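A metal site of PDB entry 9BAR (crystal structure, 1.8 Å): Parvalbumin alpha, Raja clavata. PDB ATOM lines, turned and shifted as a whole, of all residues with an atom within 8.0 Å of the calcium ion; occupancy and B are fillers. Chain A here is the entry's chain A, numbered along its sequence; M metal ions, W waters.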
ATOM      1  N   TYR A  72       2.201  -9.170  22.963  1.00  0.00           N
ATOM      2  CA  TYR A  72       1.829  -8.142  22.013  1.00  0.00           C
ATOM      3  C   TYR A  72       3.040  -7.661  21.237  1.00  0.00           C
ATOM      4  O   TYR A  72       4.168  -7.738  21.737  1.00  0.00           O
ATOM      5  CB  TYR A  72       1.212  -6.916  22.692  1.00  0.00           C
ATOM      6  CG  TYR A  72       0.133  -7.274  23.700  1.00  0.00           C
ATOM      7  CD1 TYR A  72      -1.183  -7.484  23.292  1.00  0.00           C
ATOM      8  CD2 TYR A  72       0.442  -7.442  25.042  1.00  0.00           C
ATOM      9  CE1 TYR A  72      -2.160  -7.833  24.218  1.00  0.00           C
ATOM     10  CE2 TYR A  72      -0.521  -7.774  25.971  1.00  0.00           C
ATOM     11  CZ  TYR A  72      -1.821  -7.972  25.552  1.00  0.00           C
ATOM     12  OH  TYR A  72      -2.743  -8.294  26.507  1.00  0.00           O
ATOM     13  N   ILE A  73       2.775  -7.133  20.045  1.00  0.00           N
ATOM     14  CA  ILE A  73       3.728  -6.296  19.341  1.00  0.00           C
ATOM     15  C   ILE A  73       3.403  -4.861  19.713  1.00  0.00           C
ATOM     16  O   ILE A  73       2.363  -4.340  19.293  1.00  0.00           O
ATOM     17  CB  ILE A  73       3.670  -6.527  17.819  1.00  0.00           C
ATOM     18  CG1 ILE A  73       3.843  -8.013  17.485  1.00  0.00           C
ATOM     19  CG2 ILE A  73       4.692  -5.653  17.102  1.00  0.00           C
ATOM     20  CD1 ILE A  73       3.437  -8.384  16.057  1.00  0.00           C
ATOM     21  N   LEU A 101       0.027   0.323  12.814  1.00  0.00           N
ATOM     22  CA  LEU A 101      -0.694   0.058  14.042  1.00  0.00           C
ATOM     23  C   LEU A 101      -2.193   0.174  13.810  1.00  0.00           C
ATOM     24  O   LEU A 101      -2.956  -0.669  14.281  1.00  0.00           O
ATOM     25  CB  LEU A 101      -0.226   1.012  15.129  1.00  0.00           C
ATOM     26  CG  LEU A 101      -0.926   0.854  16.469  1.00  0.00           C
ATOM     27  CD1 LEU A 101      -0.680  -0.503  17.092  1.00  0.00           C
ATOM     28  CD2 LEU A 101      -0.471   1.973  17.384  1.00  0.00           C
ATOM     29  N   GLY A 104      -3.827  -2.750  12.149  1.00  0.00           N
ATOM     30  CA  GLY A 104      -3.832  -3.987  12.912  1.00  0.00           C
ATOM     31  C   GLY A 104      -4.640  -3.908  14.206  1.00  0.00           C
ATOM     32  O   GLY A 104      -5.185  -4.923  14.657  1.00  0.00           O
ATOM     33  N   ASP A 105      -4.666  -2.729  14.844  1.00  0.00           N
ATOM     34  CA  ASP A 105      -5.166  -2.632  16.218  1.00  0.00           C
ATOM     35  C   ASP A 105      -6.671  -2.407  16.210  1.00  0.00           C
ATOM     36  O   ASP A 105      -7.134  -1.272  16.288  1.00  0.00           O
ATOM     37  CB  ASP A 105      -4.489  -1.525  17.010  1.00  0.00           C
ATOM     38  CG  ASP A 105      -4.986  -1.402  18.444  1.00  0.00           C
ATOM     39  OD1 ASP A 105      -5.304  -2.454  19.050  1.00  0.00           O
ATOM     40  OD2 ASP A 105      -5.048  -0.259  18.952  1.00  0.00           O
ATOM     41  N   SER A 106      -7.422  -3.517  16.176  1.00  0.00           N
ATOM     42  CA  SER A 106      -8.880  -3.438  16.148  1.00  0.00           C
ATOM     43  C   SER A 106      -9.487  -3.344  17.553  1.00  0.00           C
ATOM     44  O   SER A 106     -10.623  -2.899  17.694  1.00  0.00           O
ATOM     45  CB  SER A 106      -9.457  -4.606  15.392  1.00  0.00           C
ATOM     46  OG  SER A 106      -9.027  -5.844  15.960  1.00  0.00           O
ATOM     47  N   ASP A 107      -8.774  -3.759  18.602  1.00  0.00           N
ATOM     48  CA  ASP A 107      -9.382  -3.788  19.930  1.00  0.00           C
ATOM     49  C   ASP A 107      -9.022  -2.533  20.745  1.00  0.00           C
ATOM     50  O   ASP A 107      -9.430  -2.421  21.892  1.00  0.00           O
ATOM     51  CB  ASP A 107      -9.081  -5.082  20.667  1.00  0.00           C
ATOM     52  CG  ASP A 107      -7.614  -5.324  21.006  1.00  0.00           C
ATOM     53  OD1 ASP A 107      -6.833  -4.353  20.951  1.00  0.00           O
ATOM     54  OD2 ASP A 107      -7.269  -6.492  21.294  1.00  0.00           O
ATOM     55  N   GLY A 108      -8.233  -1.621  20.161  1.00  0.00           N
ATOM     56  CA  GLY A 108      -8.111  -0.261  20.663  1.00  0.00           C
ATOM     57  C   GLY A 108      -7.065  -0.074  21.767  1.00  0.00           C
ATOM     58  O   GLY A 108      -7.067   0.968  22.425  1.00  0.00           O
ATOM     59  N   ASP A 109      -6.140  -1.027  21.956  1.00  0.00           N
ATOM     60  CA  ASP A 109      -5.199  -0.941  23.074  1.00  0.00           C
ATOM     61  C   ASP A 109      -3.815  -0.476  22.608  1.00  0.00           C
ATOM     62  O   ASP A 109      -2.872  -0.506  23.394  1.00  0.00           O
ATOM     63  CB  ASP A 109      -5.084  -2.266  23.819  1.00  0.00           C
ATOM     64  CG  ASP A 109      -4.481  -3.409  23.030  1.00  0.00           C
ATOM     65  OD1 ASP A 109      -4.352  -3.282  21.777  1.00  0.00           O
ATOM     66  OD2 ASP A 109      -4.122  -4.429  23.645  1.00  0.00           O
ATOM     67  N   HIS A 110      -3.685  -0.059  21.334  1.00  0.00           N
ATOM     68  CA  HIS A 110      -2.465   0.527  20.810  1.00  0.00           C
ATOM     69  C   HIS A 110      -1.315  -0.483  20.755  1.00  0.00           C
ATOM     70  O   HIS A 110      -0.144  -0.090  20.790  1.00  0.00           O
ATOM     71  CB  HIS A 110      -2.060   1.798  21.578  1.00  0.00           C
ATOM     72  CG  HIS A 110      -3.255   2.600  21.963  1.00  0.00           C
ATOM     73  ND1 HIS A 110      -4.050   3.216  21.022  1.00  0.00           N
ATOM     74  CD2 HIS A 110      -3.841   2.803  23.142  1.00  0.00           C
ATOM     75  CE1 HIS A 110      -5.064   3.813  21.639  1.00  0.00           C
ATOM     76  NE2 HIS A 110      -4.957   3.572  22.927  1.00  0.00           N
ATOM     77  N   LYS A 111      -1.641  -1.770  20.603  1.00  0.00           N
ATOM     78  CA  LYS A 111      -0.641  -2.808  20.412  1.00  0.00           C
ATOM     79  C   LYS A 111      -1.269  -3.926  19.585  1.00  0.00           C
ATOM     80  O   LYS A 111      -2.494  -3.952  19.415  1.00  0.00           O
ATOM     81  CB  LYS A 111      -0.024  -3.262  21.745  1.00  0.00           C
ATOM     82  CG  LYS A 111      -0.988  -3.545  22.880  1.00  0.00           C
ATOM     83  CD  LYS A 111      -0.254  -3.695  24.204  1.00  0.00           C
ATOM     84  CE  LYS A 111      -1.132  -4.060  25.350  1.00  0.00           C
ATOM     85  NZ  LYS A 111      -0.344  -4.125  26.582  1.00  0.00           N
ATOM     86  N   ILE A 112      -0.453  -4.840  19.033  1.00  0.00           N
ATOM     87  CA  ILE A 112      -0.992  -5.853  18.134  1.00  0.00           C
ATOM     88  C   ILE A 112      -0.928  -7.216  18.825  1.00  0.00           C
ATOM     89  O   ILE A 112       0.147  -7.652  19.220  1.00  0.00           O
ATOM     90  CB  ILE A 112      -0.297  -5.848  16.761  1.00  0.00           C
ATOM     91  CG1 ILE A 112      -0.542  -4.531  16.029  1.00  0.00           C
ATOM     92  CG2 ILE A 112      -0.741  -7.049  15.915  1.00  0.00           C
ATOM     93  CD1 ILE A 112       0.181  -4.393  14.711  1.00  0.00           C
ATOM     94  N   GLY A 113      -2.100  -7.856  18.973  1.00  0.00           N
ATOM     95  CA  GLY A 113      -2.195  -9.179  19.581  1.00  0.00           C
ATOM     96  C   GLY A 113      -2.168 -10.275  18.520  1.00  0.00           C
ATOM     97  O   GLY A 113      -2.149  -9.981  17.339  1.00  0.00           O
ATOM     98  N   VAL A 114      -2.146 -11.537  18.963  1.00  0.00           N
ATOM     99  CA  VAL A 114      -1.964 -12.637  18.039  1.00  0.00           C
ATOM    100  C   VAL A 114      -3.146 -12.711  17.081  1.00  0.00           C
ATOM    101  O   VAL A 114      -2.944 -12.862  15.880  1.00  0.00           O
ATOM    102  CB  VAL A 114      -1.687 -13.974  18.769  1.00  0.00           C
ATOM    103  CG1 VAL A 114      -2.833 -14.413  19.693  1.00  0.00           C
ATOM    104  CG2 VAL A 114      -1.355 -15.070  17.773  1.00  0.00           C
ATOM    105  N   GLU A 116      -5.191 -10.298  16.127  1.00  0.00           N
ATOM    106  CA  GLU A 116      -5.145  -9.138  15.248  1.00  0.00           C
ATOM    107  C   GLU A 116      -4.094  -9.323  14.160  1.00  0.00           C
ATOM    108  O   GLU A 116      -4.284  -8.869  13.036  1.00  0.00           O
ATOM    109  CB  GLU A 116      -4.839  -7.867  16.047  1.00  0.00           C
ATOM    110  CG  GLU A 116      -5.957  -7.404  16.975  1.00  0.00           C
ATOM    111  CD  GLU A 116      -5.566  -6.288  17.913  1.00  0.00           C
ATOM    112  OE1 GLU A 116      -4.385  -6.276  18.365  1.00  0.00           O
ATOM    113  OE2 GLU A 116      -6.417  -5.423  18.247  1.00  0.00           O
ATOM    114  N   PHE A 117      -2.957  -9.936  14.511  1.00  0.00           N
ATOM    115  CA  PHE A 117      -1.898 -10.191  13.550  1.00  0.00           C
ATOM    116  C   PHE A 117      -2.399 -11.146  12.459  1.00  0.00           C
ATOM    117  O   PHE A 117      -2.216 -10.871  11.280  1.00  0.00           O
ATOM    118  CB  PHE A 117      -0.637 -10.721  14.230  1.00  0.00           C
ATOM    119  CG  PHE A 117       0.497 -10.970  13.255  1.00  0.00           C
ATOM    120  CD1 PHE A 117       1.205  -9.912  12.709  1.00  0.00           C
ATOM    121  CD2 PHE A 117       0.864 -12.262  12.896  1.00  0.00           C
ATOM    122  CE1 PHE A 117       2.245 -10.142  11.812  1.00  0.00           C
ATOM    123  CE2 PHE A 117       1.902 -12.487  12.012  1.00  0.00           C
ATOM    124  CZ  PHE A 117       2.588 -11.429  11.470  1.00  0.00           C
HETATM  125 CA    CA M   1      -4.743  -4.480  19.997  1.00  0.00          CA
HETATM  126  O   HOH W   1      -3.757  -6.123  21.670  1.00  0.00           O
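OD1 of Asp 105 sits close to N of Gly 108, at 3.2 Å. The side-chain carboxylate (OD2) of Asp 105 sits at hydrogen-bond distance from the backbone NH (N) of His 110 (2.8 Å). OE1 of Glu 116 sits close to N of Gly 113 (2.8 Å). The side-chain carboxylate (OE2) of Glu 116 lies close to the backbone NH (N) of Ser 106 (3.0 Å).
Within 4 Å of the calcium ion: Asp 105, Asp 107, Asp 109, Lys 111 and Glu 116. The nearest printed residue that does not touch the calcium ion is Ile 112 (4.4 Å).
The calcium ion is bound by OD1 of Asp 109 (2.2 Å), OD1 of Asp 107 (2.3 Å), OD1 of Asp 105 (2.3 Å), O of Lys 111 (2.4 Å), OE1 of Glu 116 (2.5 Å), water W1 (2.5 Å) and OE2 of Glu 116 (2.6 Å).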
